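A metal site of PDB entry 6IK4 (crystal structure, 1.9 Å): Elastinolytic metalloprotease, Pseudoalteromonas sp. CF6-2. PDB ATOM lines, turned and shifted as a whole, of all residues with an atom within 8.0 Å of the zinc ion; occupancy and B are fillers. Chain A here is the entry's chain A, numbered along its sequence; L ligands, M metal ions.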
ATOM      1  N   GLY A  19      -7.679 -29.680  32.321  1.00  0.00           N
ATOM      2  CA  GLY A  19      -8.447 -30.551  31.456  1.00  0.00           C
ATOM      3  C   GLY A  19      -8.396 -30.120  29.989  1.00  0.00           C
ATOM      4  O   GLY A  19      -8.097 -28.976  29.650  1.00  0.00           O
ATOM      5  N   ALA A  20      -8.729 -31.073  29.124  1.00  0.00           N
ATOM      6  CA  ALA A  20      -8.737 -30.807  27.686  1.00  0.00           C
ATOM      7  C   ALA A  20      -9.860 -29.832  27.330  1.00  0.00           C
ATOM      8  O   ALA A  20     -10.952 -29.878  27.900  1.00  0.00           O
ATOM      9  CB  ALA A  20      -8.886 -32.114  26.910  1.00  0.00           C
ATOM     10  N   HIS A  21      -9.565 -28.938  26.385  1.00  0.00           N
ATOM     11  CA  HIS A  21     -10.524 -27.948  25.930  1.00  0.00           C
ATOM     12  C   HIS A  21     -10.235 -27.613  24.478  1.00  0.00           C
ATOM     13  O   HIS A  21      -9.167 -27.922  23.944  1.00  0.00           O
ATOM     14  CB  HIS A  21     -10.498 -26.679  26.800  1.00  0.00           C
ATOM     15  CG  HIS A  21      -9.126 -26.099  27.017  1.00  0.00           C
ATOM     16  ND1 HIS A  21      -8.200 -26.683  27.848  1.00  0.00           N
ATOM     17  CD2 HIS A  21      -8.545 -24.985  26.510  1.00  0.00           C
ATOM     18  CE1 HIS A  21      -7.099 -25.951  27.852  1.00  0.00           C
ATOM     19  NE2 HIS A  21      -7.272 -24.920  27.044  1.00  0.00           N
ATOM     20  N   SER A  22     -11.210 -26.973  23.833  1.00  0.00           N
ATOM     21  CA  SER A  22     -10.979 -26.479  22.490  1.00  0.00           C
ATOM     22  C   SER A  22     -10.041 -25.279  22.533  1.00  0.00           C
ATOM     23  O   SER A  22      -9.769 -24.708  23.594  1.00  0.00           O
ATOM     24  CB  SER A  22     -12.293 -26.100  21.804  1.00  0.00           C
ATOM     25  OG  SER A  22     -12.658 -24.775  22.168  1.00  0.00           O
ATOM     26  N   ASN A  23      -9.592 -24.867  21.347  1.00  0.00           N
ATOM     27  CA  ASN A  23      -8.653 -23.758  21.270  1.00  0.00           C
ATOM     28  C   ASN A  23      -9.231 -22.500  21.900  1.00  0.00           C
ATOM     29  O   ASN A  23      -8.493 -21.717  22.509  1.00  0.00           O
ATOM     30  CB  ASN A  23      -8.268 -23.483  19.815  1.00  0.00           C
ATOM     31  CG  ASN A  23      -7.192 -22.420  19.707  1.00  0.00           C
ATOM     32  OD1 ASN A  23      -6.185 -22.461  20.423  1.00  0.00           O
ATOM     33  ND2 ASN A  23      -7.398 -21.455  18.817  1.00  0.00           N
ATOM     34  N   THR A  24     -10.554 -22.301  21.796  1.00  0.00           N
ATOM     35  CA  THR A  24     -11.196 -21.124  22.386  1.00  0.00           C
ATOM     36  C   THR A  24     -11.741 -21.385  23.781  1.00  0.00           C
ATOM     37  O   THR A  24     -12.029 -20.416  24.491  1.00  0.00           O
ATOM     38  CB  THR A  24     -12.367 -20.653  21.529  1.00  0.00           C
ATOM     39  OG1 THR A  24     -13.371 -21.671  21.488  1.00  0.00           O
ATOM     40  CG2 THR A  24     -11.904 -20.338  20.110  1.00  0.00           C
ATOM     41  N   GLY A  25     -11.897 -22.640  24.176  1.00  0.00           N
ATOM     42  CA  GLY A  25     -12.542 -22.970  25.423  1.00  0.00           C
ATOM     43  C   GLY A  25     -14.032 -23.221  25.311  1.00  0.00           C
ATOM     44  O   GLY A  25     -14.658 -23.546  26.325  1.00  0.00           O
ATOM     45  N   SER A  32      -6.766 -28.965  23.196  1.00  0.00           N
ATOM     46  CA  SER A  32      -5.795 -28.133  23.879  1.00  0.00           C
ATOM     47  C   SER A  32      -5.691 -28.497  25.357  1.00  0.00           C
ATOM     48  O   SER A  32      -6.633 -28.995  25.965  1.00  0.00           O
ATOM     49  CB  SER A  32      -6.163 -26.646  23.740  1.00  0.00           C
ATOM     50  OG  SER A  32      -6.285 -26.264  22.380  1.00  0.00           O
ATOM     51  N   LEU A  33      -4.512 -28.213  25.929  1.00  0.00           N
ATOM     52  CA  LEU A  33      -4.230 -28.374  27.347  1.00  0.00           C
ATOM     53  C   LEU A  33      -3.493 -27.139  27.819  1.00  0.00           C
ATOM     54  O   LEU A  33      -2.684 -26.567  27.085  1.00  0.00           O
ATOM     55  CB  LEU A  33      -3.363 -29.622  27.620  1.00  0.00           C
ATOM     56  CG  LEU A  33      -4.009 -30.964  27.286  1.00  0.00           C
ATOM     57  CD1 LEU A  33      -2.930 -32.038  27.109  1.00  0.00           C
ATOM     58  CD2 LEU A  33      -4.996 -31.375  28.382  1.00  0.00           C
ATOM     59  N   ASP A  34      -3.760 -26.718  29.063  1.00  0.00           N
ATOM     60  CA  ASP A  34      -3.004 -25.632  29.684  1.00  0.00           C
ATOM     61  C   ASP A  34      -1.983 -26.244  30.652  1.00  0.00           C
ATOM     62  O   ASP A  34      -2.364 -26.958  31.585  1.00  0.00           O
ATOM     63  CB  ASP A  34      -3.945 -24.665  30.419  1.00  0.00           C
ATOM     64  CG  ASP A  34      -4.883 -23.962  29.471  1.00  0.00           C
ATOM     65  OD1 ASP A  34      -4.545 -23.859  28.276  1.00  0.00           O
ATOM     66  OD2 ASP A  34      -5.957 -23.495  29.900  1.00  0.00           O
ATOM     67  N   PHE A  35      -0.694 -25.998  30.402  1.00  0.00           N
ATOM     68  CA  PHE A  35       0.401 -26.511  31.213  1.00  0.00           C
ATOM     69  C   PHE A  35       1.055 -25.398  32.019  1.00  0.00           C
ATOM     70  O   PHE A  35       1.272 -24.301  31.484  1.00  0.00           O
ATOM     71  CB  PHE A  35       1.509 -27.143  30.363  1.00  0.00           C
ATOM     72  CG  PHE A  35       1.104 -28.364  29.591  1.00  0.00           C
ATOM     73  CD1 PHE A  35       0.386 -29.387  30.189  1.00  0.00           C
ATOM     74  CD2 PHE A  35       1.466 -28.496  28.262  1.00  0.00           C
ATOM     75  CE1 PHE A  35       0.038 -30.517  29.486  1.00  0.00           C
ATOM     76  CE2 PHE A  35       1.119 -29.623  27.536  1.00  0.00           C
ATOM     77  CZ  PHE A  35       0.417 -30.637  28.146  1.00  0.00           C
ATOM     78  N   TYR A  78       0.568 -21.047  22.830  1.00  0.00           N
ATOM     79  CA  TYR A  78       0.022 -19.704  22.990  1.00  0.00           C
ATOM     80  C   TYR A  78       0.228 -19.219  24.430  1.00  0.00           C
ATOM     81  O   TYR A  78       0.459 -20.023  25.337  1.00  0.00           O
ATOM     82  CB  TYR A  78      -1.464 -19.655  22.579  1.00  0.00           C
ATOM     83  CG  TYR A  78      -2.033 -18.257  22.555  1.00  0.00           C
ATOM     84  CD1 TYR A  78      -1.568 -17.313  21.651  1.00  0.00           C
ATOM     85  CD2 TYR A  78      -3.015 -17.867  23.456  1.00  0.00           C
ATOM     86  CE1 TYR A  78      -2.075 -16.003  21.636  1.00  0.00           C
ATOM     87  CE2 TYR A  78      -3.528 -16.569  23.444  1.00  0.00           C
ATOM     88  CZ  TYR A  78      -3.044 -15.646  22.529  1.00  0.00           C
ATOM     89  OH  TYR A  78      -3.556 -14.354  22.530  1.00  0.00           O
ATOM     90  N   HIS A  79       0.187 -17.886  24.601  1.00  0.00           N
ATOM     91  CA  HIS A  79       0.557 -17.188  25.845  1.00  0.00           C
ATOM     92  C   HIS A  79       2.080 -17.170  26.050  1.00  0.00           C
ATOM     93  O   HIS A  79       2.553 -17.256  27.183  1.00  0.00           O
ATOM     94  CB  HIS A  79      -0.113 -17.772  27.094  1.00  0.00           C
ATOM     95  CG  HIS A  79      -1.600 -17.890  27.005  1.00  0.00           C
ATOM     96  ND1 HIS A  79      -2.415 -16.827  26.674  1.00  0.00           N
ATOM     97  CD2 HIS A  79      -2.422 -18.929  27.276  1.00  0.00           C
ATOM     98  CE1 HIS A  79      -3.678 -17.213  26.717  1.00  0.00           C
ATOM     99  NE2 HIS A  79      -3.716 -18.491  27.069  1.00  0.00           N
ATOM    100  N   GLN A 113      -8.305 -15.122  27.328  1.00  0.00           N
ATOM    101  CA  GLN A 113      -8.386 -14.878  28.764  1.00  0.00           C
ATOM    102  C   GLN A 113      -7.394 -15.789  29.479  1.00  0.00           C
ATOM    103  O   GLN A 113      -7.035 -16.856  28.977  1.00  0.00           O
ATOM    104  CB  GLN A 113      -9.791 -15.114  29.308  1.00  0.00           C
ATOM    105  CG  GLN A 113     -10.536 -16.287  28.685  1.00  0.00           C
ATOM    106  CD  GLN A 113     -11.919 -16.483  29.285  1.00  0.00           C
ATOM    107  OE1 GLN A 113     -12.132 -17.414  30.067  1.00  0.00           O
ATOM    108  NE2 GLN A 113     -12.865 -15.610  28.924  1.00  0.00           N
ATOM    109  N   HIS A 118       0.717 -19.651  32.042  1.00  0.00           N
ATOM    110  CA  HIS A 118       0.687 -21.032  31.549  1.00  0.00           C
ATOM    111  C   HIS A 118       0.897 -20.969  30.041  1.00  0.00           C
ATOM    112  O   HIS A 118       0.791 -19.907  29.430  1.00  0.00           O
ATOM    113  CB  HIS A 118      -0.640 -21.723  31.871  1.00  0.00           C
ATOM    114  CG  HIS A 118      -1.811 -21.163  31.125  1.00  0.00           C
ATOM    115  ND1 HIS A 118      -2.467 -20.019  31.529  1.00  0.00           N
ATOM    116  CD2 HIS A 118      -2.443 -21.584  30.004  1.00  0.00           C
ATOM    117  CE1 HIS A 118      -3.465 -19.764  30.692  1.00  0.00           C
ATOM    118  NE2 HIS A 118      -3.466 -20.704  29.753  1.00  0.00           N
ATOM    119  N   VAL A 119       1.175 -22.113  29.440  1.00  0.00           N
ATOM    120  CA  VAL A 119       1.148 -22.231  27.983  1.00  0.00           C
ATOM    121  C   VAL A 119      -0.131 -22.962  27.589  1.00  0.00           C
ATOM    122  O   VAL A 119      -0.490 -23.977  28.195  1.00  0.00           O
ATOM    123  CB  VAL A 119       2.394 -22.937  27.432  1.00  0.00           C
ATOM    124  CG1 VAL A 119       2.592 -24.318  28.069  1.00  0.00           C
ATOM    125  CG2 VAL A 119       2.295 -23.074  25.902  1.00  0.00           C
ATOM    126  N   HIS A 120      -0.852 -22.411  26.617  1.00  0.00           N
ATOM    127  CA  HIS A 120      -2.000 -23.032  25.990  1.00  0.00           C
ATOM    128  C   HIS A 120      -1.464 -23.862  24.827  1.00  0.00           C
ATOM    129  O   HIS A 120      -0.981 -23.301  23.846  1.00  0.00           O
ATOM    130  CB  HIS A 120      -2.991 -21.953  25.531  1.00  0.00           C
ATOM    131  CG  HIS A 120      -4.110 -22.446  24.664  1.00  0.00           C
ATOM    132  ND1 HIS A 120      -5.263 -22.989  25.189  1.00  0.00           N
ATOM    133  CD2 HIS A 120      -4.288 -22.413  23.320  1.00  0.00           C
ATOM    134  CE1 HIS A 120      -6.103 -23.282  24.198  1.00  0.00           C
ATOM    135  NE2 HIS A 120      -5.523 -22.945  23.053  1.00  0.00           N
ATOM    136  N   PHE A 121      -1.519 -25.185  24.964  1.00  0.00           N
ATOM    137  CA  PHE A 121      -0.897 -26.139  24.041  1.00  0.00           C
ATOM    138  C   PHE A 121      -1.971 -26.826  23.214  1.00  0.00           C
ATOM    139  O   PHE A 121      -2.903 -27.396  23.772  1.00  0.00           O
ATOM    140  CB  PHE A 121      -0.101 -27.156  24.878  1.00  0.00           C
ATOM    141  CG  PHE A 121       0.492 -28.300  24.097  1.00  0.00           C
ATOM    142  CD1 PHE A 121       1.731 -28.177  23.490  1.00  0.00           C
ATOM    143  CD2 PHE A 121      -0.158 -29.528  24.058  1.00  0.00           C
ATOM    144  CE1 PHE A 121       2.299 -29.246  22.807  1.00  0.00           C
ATOM    145  CE2 PHE A 121       0.401 -30.600  23.374  1.00  0.00           C
ATOM    146  CZ  PHE A 121       1.626 -30.466  22.750  1.00  0.00           C
ATOM    147  N   THR A 122      -1.824 -26.806  21.878  1.00  0.00           N
ATOM    148  CA  THR A 122      -2.876 -27.270  20.973  1.00  0.00           C
ATOM    149  C   THR A 122      -2.305 -28.230  19.934  1.00  0.00           C
ATOM    150  O   THR A 122      -1.249 -27.968  19.374  1.00  0.00           O
ATOM    151  CB  THR A 122      -3.556 -26.096  20.238  1.00  0.00           C
ATOM    152  OG1 THR A 122      -4.061 -25.149  21.187  1.00  0.00           O
ATOM    153  CG2 THR A 122      -4.705 -26.569  19.273  1.00  0.00           C
ATOM    154  N   TYR A 149     -12.537 -28.099  29.641  1.00  0.00           N
ATOM    155  CA  TYR A 149     -11.757 -27.967  30.875  1.00  0.00           C
ATOM    156  C   TYR A 149     -12.157 -28.958  31.947  1.00  0.00           C
ATOM    157  O   TYR A 149     -11.694 -28.842  33.089  1.00  0.00           O
ATOM    158  CB  TYR A 149     -11.853 -26.557  31.460  1.00  0.00           C
ATOM    159  CG  TYR A 149     -11.346 -25.436  30.572  1.00  0.00           C
ATOM    160  CD1 TYR A 149      -9.977 -25.201  30.428  1.00  0.00           C
ATOM    161  CD2 TYR A 149     -12.236 -24.611  29.895  1.00  0.00           C
ATOM    162  CE1 TYR A 149      -9.514 -24.160  29.631  1.00  0.00           C
ATOM    163  CE2 TYR A 149     -11.780 -23.576  29.088  1.00  0.00           C
ATOM    164  CZ  TYR A 149     -10.428 -23.354  28.955  1.00  0.00           C
ATOM    165  OH  TYR A 149      -9.993 -22.323  28.155  1.00  0.00           O
HETATM  166  C1  LIG L   1      -6.369 -20.718  28.274  1.00  0.00           C
HETATM  167  O1  LIG L   1      -4.993 -20.498  28.115  1.00  0.00           O
HETATM  168  C2  LIG L   1      -6.986 -20.944  26.923  1.00  0.00           C
HETATM  169  O2  LIG L   1      -7.900 -22.006  27.011  1.00  0.00           O
HETATM  170  C3  LIG L   1      -7.637 -19.650  26.444  1.00  0.00           C
HETATM  171  O3  LIG L   1      -6.642 -18.766  25.948  1.00  0.00           O
HETATM  172 ZN    ZN M   1      -6.046 -23.217  27.070  1.00  0.00          ZN
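Within 4 Å of the zinc ion: His 21, Asp 34 and His 120.
A ring nitrogen (NE2) of His 120 lies within hydrogen-bond range of the side-chain hydroxyl (OG) of Ser 32 (3.5 Å). NE2 of His 120 is in hydrogen-bond range of OD1 of Asn 23, at 2.8 Å. A ring nitrogen (NE2) of His 120 is in hydrogen-bond range of the side-chain hydroxyl (OG1) of Thr 122 (3.2 Å). The backbone carbonyl oxygen (O) of His 120 sits at hydrogen-bond distance from the backbone NH (N) of Tyr 78, at 2.9 Å. O of His 21 is in hydrogen-bond range of N of Ser 32 (2.7 Å). ND1 of His 21 sits at hydrogen-bond distance from O of Gly 19 (2.9 Å).
OD1 of Asp 34 is bound to the zinc ion. A ring nitrogen (ND1) of His 120 is bound to the zinc ion (2.1 Å). A ring nitrogen (NE2) of His 21 is bound to the zinc ion. O2 of the ligand binds the zinc ion (2.2 Å). Slightly farther from the zinc ion lies the side-chain carboxylate (OD2) of Asp 34 (2.8 Å).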
